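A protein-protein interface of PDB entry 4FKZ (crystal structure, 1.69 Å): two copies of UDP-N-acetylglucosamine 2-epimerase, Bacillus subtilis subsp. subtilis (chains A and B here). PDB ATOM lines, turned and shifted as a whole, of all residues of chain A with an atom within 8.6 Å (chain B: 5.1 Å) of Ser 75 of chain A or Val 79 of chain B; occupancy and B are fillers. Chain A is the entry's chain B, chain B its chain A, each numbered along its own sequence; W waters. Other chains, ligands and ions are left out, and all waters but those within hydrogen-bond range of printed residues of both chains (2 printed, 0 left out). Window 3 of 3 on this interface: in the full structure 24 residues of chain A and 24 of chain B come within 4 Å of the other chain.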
ATOM      1  N   ILE A  63       3.062   2.619  18.539  1.00  0.00           N
ATOM      2  CA  ILE A  63       3.522   2.820  19.916  1.00  0.00           C
ATOM      3  C   ILE A  63       2.600   3.650  20.805  1.00  0.00           C
ATOM      4  O   ILE A  63       2.746   3.609  22.030  1.00  0.00           O
ATOM      5  CB  ILE A  63       4.976   3.390  20.020  1.00  0.00           C
ATOM      6  CG1 ILE A  63       5.039   4.883  19.663  1.00  0.00           C
ATOM      7  CG2 ILE A  63       5.951   2.534  19.208  1.00  0.00           C
ATOM      8  CD1 ILE A  63       6.408   5.517  19.897  1.00  0.00           C
ATOM      9  N   THR A  69       4.071   9.486  28.536  1.00  0.00           N
ATOM     10  CA  THR A  69       5.120  10.383  28.999  1.00  0.00           C
ATOM     11  C   THR A  69       6.276  10.389  28.000  1.00  0.00           C
ATOM     12  O   THR A  69       6.362   9.511  27.133  1.00  0.00           O
ATOM     13  CB  THR A  69       5.662   9.942  30.377  1.00  0.00           C
ATOM     14  OG1 THR A  69       6.292   8.668  30.255  1.00  0.00           O
ATOM     15  CG2 THR A  69       4.536   9.862  31.405  1.00  0.00           C
ATOM     16  N   LEU A  70       7.156  11.381  28.126  1.00  0.00           N
ATOM     17  CA  LEU A  70       8.381  11.434  27.314  1.00  0.00           C
ATOM     18  C   LEU A  70       9.224  10.162  27.430  1.00  0.00           C
ATOM     19  O   LEU A  70       9.690   9.617  26.415  1.00  0.00           O
ATOM     20  CB  LEU A  70       9.199  12.690  27.657  1.00  0.00           C
ATOM     21  CG  LEU A  70       8.503  14.027  27.359  1.00  0.00           C
ATOM     22  CD1 LEU A  70       9.384  15.195  27.793  1.00  0.00           C
ATOM     23  CD2 LEU A  70       8.094  14.170  25.889  1.00  0.00           C
ATOM     24  N   ALA A  71       9.408   9.677  28.664  1.00  0.00           N
ATOM     25  CA  ALA A  71      10.112   8.431  28.877  1.00  0.00           C
ATOM     26  C   ALA A  71       9.463   7.253  28.154  1.00  0.00           C
ATOM     27  O   ALA A  71      10.169   6.451  27.577  1.00  0.00           O
ATOM     28  CB  ALA A  71      10.254   8.137  30.373  1.00  0.00           C
ATOM     29  N   GLU A  72       8.125   7.165  28.196  1.00  0.00           N
ATOM     30  CA  GLU A  72       7.402   6.111  27.514  1.00  0.00           C
ATOM     31  C   GLU A  72       7.582   6.163  25.999  1.00  0.00           C
ATOM     32  O   GLU A  72       7.870   5.143  25.386  1.00  0.00           O
ATOM     33  CB  GLU A  72       5.918   6.162  27.874  1.00  0.00           C
ATOM     34  CG  GLU A  72       5.647   5.532  29.227  1.00  0.00           C
ATOM     35  CD  GLU A  72       4.199   5.666  29.658  1.00  0.00           C
ATOM     36  OE1 GLU A  72       3.540   6.670  29.302  1.00  0.00           O
ATOM     37  OE2 GLU A  72       3.723   4.753  30.373  1.00  0.00           O
ATOM     38  N   ILE A  73       7.417   7.334  25.396  1.00  0.00           N
ATOM     39  CA  ILE A  73       7.606   7.442  23.936  1.00  0.00           C
ATOM     40  C   ILE A  73       9.030   7.017  23.583  1.00  0.00           C
ATOM     41  O   ILE A  73       9.251   6.224  22.656  1.00  0.00           O
ATOM     42  CB  ILE A  73       7.384   8.872  23.382  1.00  0.00           C
ATOM     43  CG1 ILE A  73       6.012   9.431  23.770  1.00  0.00           C
ATOM     44  CG2 ILE A  73       7.566   8.883  21.864  1.00  0.00           C
ATOM     45  CD1 ILE A  73       5.883  10.942  23.643  1.00  0.00           C
ATOM     46  N   THR A  74       9.999   7.542  24.339  1.00  0.00           N
ATOM     47  CA  THR A  74      11.418   7.295  24.030  1.00  0.00           C
ATOM     48  C   THR A  74      11.740   5.812  24.099  1.00  0.00           C
ATOM     49  O   THR A  74      12.331   5.256  23.183  1.00  0.00           O
ATOM     50  CB  THR A  74      12.348   8.067  24.985  1.00  0.00           C
ATOM     51  OG1 THR A  74      11.972   9.448  25.018  1.00  0.00           O
ATOM     52  CG2 THR A  74      13.828   7.938  24.526  1.00  0.00           C
ATOM     53  N   SER A  75      11.339   5.161  25.194  1.00  0.00           N
ATOM     54  CA  SER A  75      11.586   3.745  25.377  1.00  0.00           C
ATOM     55  C   SER A  75      10.855   2.896  24.329  1.00  0.00           C
ATOM     56  O   SER A  75      11.446   2.000  23.734  1.00  0.00           O
ATOM     57  CB  SER A  75      11.155   3.317  26.789  1.00  0.00           C
ATOM     58  OG  SER A  75      11.341   1.927  26.971  1.00  0.00           O
ATOM     59  N   ASN A  76       9.562   3.158  24.137  1.00  0.00           N
ATOM     60  CA  ASN A  76       8.779   2.367  23.194  1.00  0.00           C
ATOM     61  C   ASN A  76       9.320   2.485  21.771  1.00  0.00           C
ATOM     62  O   ASN A  76       9.506   1.475  21.089  1.00  0.00           O
ATOM     63  CB  ASN A  76       7.287   2.733  23.261  1.00  0.00           C
ATOM     64  CG  ASN A  76       6.634   2.283  24.562  1.00  0.00           C
ATOM     65  OD1 ASN A  76       7.023   1.272  25.141  1.00  0.00           O
ATOM     66  ND2 ASN A  76       5.620   3.017  25.010  1.00  0.00           N
ATOM     67  N   ALA A  77       9.620   3.709  21.355  1.00  0.00           N
ATOM     68  CA  ALA A  77      10.144   3.936  20.007  1.00  0.00           C
ATOM     69  C   ALA A  77      11.511   3.284  19.851  1.00  0.00           C
ATOM     70  O   ALA A  77      11.771   2.604  18.856  1.00  0.00           O
ATOM     71  CB  ALA A  77      10.213   5.422  19.693  1.00  0.00           C
ATOM     72  N   LEU A  78      12.378   3.481  20.845  1.00  0.00           N
ATOM     73  CA  LEU A  78      13.724   2.904  20.809  1.00  0.00           C
ATOM     74  C   LEU A  78      13.711   1.380  20.717  1.00  0.00           C
ATOM     75  O   LEU A  78      14.399   0.800  19.884  1.00  0.00           O
ATOM     76  CB  LEU A  78      14.546   3.341  22.039  1.00  0.00           C
ATOM     77  CG  LEU A  78      16.003   2.860  22.105  1.00  0.00           C
ATOM     78  CD1 LEU A  78      16.789   3.307  20.881  1.00  0.00           C
ATOM     79  CD2 LEU A  78      16.662   3.377  23.368  1.00  0.00           C
ATOM     80  N   VAL A  79      12.935   0.736  21.580  1.00  0.00           N
ATOM     81  CA  VAL A  79      12.940  -0.719  21.647  1.00  0.00           C
ATOM     82  C   VAL A  79      12.383  -1.330  20.350  1.00  0.00           C
ATOM     83  O   VAL A  79      12.942  -2.302  19.826  1.00  0.00           O
ATOM     84  CB  VAL A  79      12.194  -1.212  22.903  1.00  0.00           C
ATOM     85  CG1 VAL A  79      11.875  -2.696  22.825  1.00  0.00           C
ATOM     86  CG2 VAL A  79      13.011  -0.862  24.159  1.00  0.00           C
ATOM     87  N   ARG A  80      11.300  -0.747  19.836  1.00  0.00           N
ATOM     88  CA  ARG A  80      10.668  -1.252  18.618  1.00  0.00           C
ATOM     89  C   ARG A  80      11.509  -1.005  17.355  1.00  0.00           C
ATOM     90  O   ARG A  80      11.563  -1.858  16.468  1.00  0.00           O
ATOM     91  CB  ARG A  80       9.244  -0.677  18.452  1.00  0.00           C
ATOM     92  CG  ARG A  80       8.233  -1.119  19.522  1.00  0.00           C
ATOM     93  CD  ARG A  80       7.881  -2.607  19.481  1.00  0.00           C
ATOM     94  NE  ARG A  80       7.665  -3.122  18.126  1.00  0.00           N
ATOM     95  CZ  ARG A  80       6.498  -3.135  17.478  1.00  0.00           C
ATOM     96  NH1 ARG A  80       5.393  -2.664  18.047  1.00  0.00           N
ATOM     97  NH2 ARG A  80       6.439  -3.633  16.249  1.00  0.00           N
ATOM     98  N   LEU A  81      12.152   0.159  17.271  1.00  0.00           N
ATOM     99  CA  LEU A  81      13.037   0.447  16.143  1.00  0.00           C
ATOM    100  C   LEU A  81      14.291  -0.411  16.188  1.00  0.00           C
ATOM    101  O   LEU A  81      14.778  -0.866  15.150  1.00  0.00           O
ATOM    102  CB  LEU A  81      13.403   1.934  16.085  1.00  0.00           C
ATOM    103  CG  LEU A  81      12.284   2.829  15.547  1.00  0.00           C
ATOM    104  CD1 LEU A  81      12.515   4.280  15.904  1.00  0.00           C
ATOM    105  CD2 LEU A  81      12.120   2.639  14.038  1.00  0.00           C
ATOM    106  N   ASP A  82      14.834  -0.607  17.394  1.00  0.00           N
ATOM    107  CA  ASP A  82      15.980  -1.493  17.574  1.00  0.00           C
ATOM    108  C   ASP A  82      15.640  -2.895  17.056  1.00  0.00           C
ATOM    109  O   ASP A  82      16.434  -3.486  16.331  1.00  0.00           O
ATOM    110  CB  ASP A  82      16.399  -1.526  19.055  1.00  0.00           C
ATOM    111  CG  ASP A  82      17.452  -2.578  19.350  1.00  0.00           C
ATOM    112  OD1 ASP A  82      18.617  -2.365  18.985  1.00  0.00           O
ATOM    113  OD2 ASP A  82      17.115  -3.606  19.978  1.00  0.00           O
ATOM    114  N   THR A 100       9.935  13.394  19.716  1.00  0.00           N
ATOM    115  CA  THR A 100      10.627  12.328  20.415  1.00  0.00           C
ATOM    116  C   THR A 100      10.895  11.145  19.486  1.00  0.00           C
ATOM    117  O   THR A 100      11.918  10.463  19.628  1.00  0.00           O
ATOM    118  CB  THR A 100       9.905  11.965  21.734  1.00  0.00           C
ATOM    119  OG1 THR A 100       9.904  13.130  22.556  1.00  0.00           O
ATOM    120  CG2 THR A 100      10.607  10.841  22.465  1.00  0.00           C
ATOM    121  N   ALA A 104      14.483   9.400  19.057  1.00  0.00           N
ATOM    122  CA  ALA A 104      14.554   7.948  19.229  1.00  0.00           C
ATOM    123  C   ALA A 104      14.945   7.210  17.949  1.00  0.00           C
ATOM    124  O   ALA A 104      15.683   6.230  18.002  1.00  0.00           O
ATOM    125  CB  ALA A 104      13.232   7.407  19.784  1.00  0.00           C
ATOM    126  N   LEU A 107      18.639   7.757  17.357  1.00  0.00           N
ATOM    127  CA  LEU A 107      19.400   7.000  18.344  1.00  0.00           C
ATOM    128  C   LEU A 107      19.408   5.508  18.014  1.00  0.00           C
ATOM    129  O   LEU A 107      20.464   4.853  18.071  1.00  0.00           O
ATOM    130  CB  LEU A 107      18.854   7.263  19.751  1.00  0.00           C
ATOM    131  CG  LEU A 107      19.669   6.669  20.908  1.00  0.00           C
ATOM    132  CD1 LEU A 107      20.951   7.463  21.091  1.00  0.00           C
ATOM    133  CD2 LEU A 107      18.822   6.697  22.179  1.00  0.00           C
ATOM    134  N   THR B  74      19.800   1.593  27.593  1.00  0.00           N
ATOM    135  CA  THR B  74      19.171   2.914  27.496  1.00  0.00           C
ATOM    136  C   THR B  74      17.737   2.880  28.010  1.00  0.00           C
ATOM    137  O   THR B  74      17.351   3.736  28.792  1.00  0.00           O
ATOM    138  CB  THR B  74      19.145   3.428  26.051  1.00  0.00           C
ATOM    139  OG1 THR B  74      20.483   3.408  25.526  1.00  0.00           O
ATOM    140  CG2 THR B  74      18.603   4.879  26.001  1.00  0.00           C
ATOM    141  N   SER B  75      16.972   1.898  27.538  1.00  0.00           N
ATOM    142  CA  SER B  75      15.576   1.739  27.940  1.00  0.00           C
ATOM    143  C   SER B  75      15.457   1.447  29.429  1.00  0.00           C
ATOM    144  O   SER B  75      14.692   2.110  30.129  1.00  0.00           O
ATOM    145  CB  SER B  75      14.901   0.631  27.131  1.00  0.00           C
ATOM    146  OG  SER B  75      13.528   0.566  27.497  1.00  0.00           O
ATOM    147  N   ASN B  76      16.213   0.463  29.906  1.00  0.00           N
ATOM    148  CA  ASN B  76      16.144   0.064  31.324  1.00  0.00           C
ATOM    149  C   ASN B  76      16.547   1.199  32.258  1.00  0.00           C
ATOM    150  O   ASN B  76      15.868   1.472  33.250  1.00  0.00           O
ATOM    151  CB  ASN B  76      16.988  -1.182  31.580  1.00  0.00           C
ATOM    152  CG  ASN B  76      16.420  -2.413  30.908  1.00  0.00           C
ATOM    153  OD1 ASN B  76      15.202  -2.518  30.698  1.00  0.00           O
ATOM    154  ND2 ASN B  76      17.286  -3.362  30.581  1.00  0.00           N
ATOM    155  N   ALA B  77      17.639   1.890  31.933  1.00  0.00           N
ATOM    156  CA  ALA B  77      18.058   3.019  32.746  1.00  0.00           C
ATOM    157  C   ALA B  77      17.037   4.172  32.711  1.00  0.00           C
ATOM    158  O   ALA B  77      16.682   4.728  33.751  1.00  0.00           O
ATOM    159  CB  ALA B  77      19.441   3.503  32.312  1.00  0.00           C
ATOM    160  N   LEU B  78      16.541   4.510  31.521  1.00  0.00           N
ATOM    161  CA  LEU B  78      15.585   5.608  31.393  1.00  0.00           C
ATOM    162  C   LEU B  78      14.277   5.343  32.148  1.00  0.00           C
ATOM    163  O   LEU B  78      13.796   6.215  32.869  1.00  0.00           O
ATOM    164  CB  LEU B  78      15.285   5.885  29.917  1.00  0.00           C
ATOM    165  CG  LEU B  78      14.280   6.999  29.652  1.00  0.00           C
ATOM    166  CD1 LEU B  78      14.732   8.341  30.224  1.00  0.00           C
ATOM    167  CD2 LEU B  78      14.028   7.060  28.149  1.00  0.00           C
ATOM    168  N   VAL B  79      13.726   4.149  31.970  1.00  0.00           N
ATOM    169  CA  VAL B  79      12.443   3.795  32.607  1.00  0.00           C
ATOM    170  C   VAL B  79      12.566   3.799  34.137  1.00  0.00           C
ATOM    171  O   VAL B  79      11.713   4.366  34.825  1.00  0.00           O
ATOM    172  CB  VAL B  79      11.901   2.459  32.058  1.00  0.00           C
ATOM    173  CG1 VAL B  79      10.735   1.946  32.901  1.00  0.00           C
ATOM    174  CG2 VAL B  79      11.452   2.663  30.607  1.00  0.00           C
ATOM    175  N   ARG B  80      13.634   3.189  34.653  1.00  0.00           N
ATOM    176  CA  ARG B  80      13.855   3.143  36.107  1.00  0.00           C
ATOM    177  C   ARG B  80      14.187   4.509  36.728  1.00  0.00           C
ATOM    178  O   ARG B  80      13.734   4.831  37.836  1.00  0.00           O
ATOM    179  CB  ARG B  80      14.921   2.094  36.485  1.00  0.00           C
ATOM    180  CG  ARG B  80      14.559   0.646  36.166  1.00  0.00           C
ATOM    181  CD  ARG B  80      13.431   0.144  37.053  1.00  0.00           C
ATOM    182  NE  ARG B  80      13.040  -1.229  36.731  1.00  0.00           N
ATOM    183  CZ  ARG B  80      11.927  -1.824  37.166  1.00  0.00           C
ATOM    184  NH1 ARG B  80      11.068  -1.172  37.945  1.00  0.00           N
ATOM    185  NH2 ARG B  80      11.667  -3.081  36.818  1.00  0.00           N
ATOM    186  N   LEU B  81      14.975   5.318  36.023  1.00  0.00           N
ATOM    187  CA  LEU B  81      15.255   6.671  36.495  1.00  0.00           C
ATOM    188  C   LEU B  81      14.025   7.566  36.417  1.00  0.00           C
ATOM    189  O   LEU B  81      13.805   8.403  37.293  1.00  0.00           O
ATOM    190  CB  LEU B  81      16.432   7.293  35.732  1.00  0.00           C
ATOM    191  CG  LEU B  81      17.795   6.710  36.139  1.00  0.00           C
ATOM    192  CD1 LEU B  81      18.860   6.913  35.051  1.00  0.00           C
ATOM    193  CD2 LEU B  81      18.240   7.254  37.499  1.00  0.00           C
ATOM    194  N   ASP B  82      13.224   7.397  35.364  1.00  0.00           N
ATOM    195  CA  ASP B  82      11.989   8.150  35.230  1.00  0.00           C
ATOM    196  C   ASP B  82      11.092   7.876  36.435  1.00  0.00           C
ATOM    197  O   ASP B  82      10.538   8.810  37.007  1.00  0.00           O
ATOM    198  CB  ASP B  82      11.261   7.770  33.926  1.00  0.00           C
ATOM    199  CG  ASP B  82       9.894   8.433  33.799  1.00  0.00           C
ATOM    200  OD1 ASP B  82       9.832   9.648  33.594  1.00  0.00           O
ATOM    201  OD2 ASP B  82       8.883   7.718  33.878  1.00  0.00           O
ATOM    202  N   GLU B  83      10.990   6.610  36.821  1.00  0.00           N
ATOM    203  CA  GLU B  83      10.149   6.218  37.955  1.00  0.00           C
ATOM    204  C   GLU B  83      10.675   6.843  39.248  1.00  0.00           C
ATOM    205  O   GLU B  83       9.900   7.334  40.077  1.00  0.00           O
ATOM    206  CB  GLU B  83      10.063   4.688  38.056  1.00  0.00           C
ATOM    207  CG  GLU B  83       9.148   4.158  39.168  1.00  0.00           C
ATOM    208  CD  GLU B  83       7.669   4.466  38.949  1.00  0.00           C
ATOM    209  OE1 GLU B  83       7.272   4.829  37.819  1.00  0.00           O
ATOM    210  OE2 GLU B  83       6.888   4.339  39.923  1.00  0.00           O
HETATM  211  O   HOH W   1       9.029  11.080  31.188  1.00  0.00           O
HETATM  212  O   HOH W   2       6.915   7.225  32.334  1.00  0.00           O
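Printed residues of chain B within 4 Å of Ala 71 of chain A: Leu 78 (3.9 Å) and Asp 82 (3.5 Å). Of the printed residues of chain B, Thr 74 of chain A touches Leu 78 (3.7 Å). Ser 75 of chain A touches just these residues of chain B: Ser 75 (2.6 Å) and Val 79 (3.7 Å). Thr 100 of chain A touches none of the printed residues of chain B. Printed residues of chain A within 4 Å of Thr 74 of chain B: Leu 78. Ala 77 of chain B touches none of the printed residues of chain A. Of the printed residues of chain A, Leu 78 of chain B touches Ala 71 and Thr 74. The nearest residue of chain B that does not touch Ser 75 of chain A is Leu 78 of chain B (4.4 Å).
Thr 74 of chain A touches Leu 78 of chain B, and with the chains exchanged Leu 78 of chain A touches Thr 74 of chain B. Ser 75 of chain A touches its own counterpart, Ser 75 of chain B. Ser 75 of chain A touches Val 79 of chain B, and with the chains exchanged Val 79 of chain A touches Ser 75 of chain B. 9 positions are printed for both chains.
Printed residues of chain B that touch a printed residue of chain A: Thr 74, Ser 75, Leu 78, Val 79 and Asp 82. Of the 18 printed residues of chain A, 5 touch a printed residue of chain B. Hydrophobic or aromatic side chains of chain A within 4 Å of the printed part of chain B: Ala 71, Leu 78 and Val 79. Among the printed residues, no Asp or Glu carboxylate lies within 4 Å of a Lys or Arg side-chain nitrogen of the other chain.
Water W2 bridges the side-chain carboxylate (OD2) of Asp 82 of chain B and the side-chain hydroxyl (OG1) of Thr 69 of chain A. Water W1 lies within hydrogen-bond range of N of Ala 71 of chain A (2.9 Å) and OD1 of Asp 82 of chain B (2.9 Å).
Among the printed residues, merely in contact across the chains: Ala 71 of chain A with Leu 78 of chain B (3.9 Å), Ala 71 of chain A with Asp 82 of chain B (3.5 Å), Thr 74 of chain A with Leu 78 of chain B (3.7 Å), Ser 75 of chain A with Val 79 of chain B (3.7 Å), Leu 78 of chain A with Thr 74 of chain B (3.6 Å) and Val 79 of chain A with Ser 75 of chain B (3.7 Å).
O of Leu 70 of chain A lies within hydrogen-bond range of OG1 of Thr 74 of chain A (2.7 Å).
The side-chain hydroxyl (OG) of Ser 75 of chain A is in hydrogen-bond range of the side-chain hydroxyl (OG) of Ser 75 of chain B (2.6 Å).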
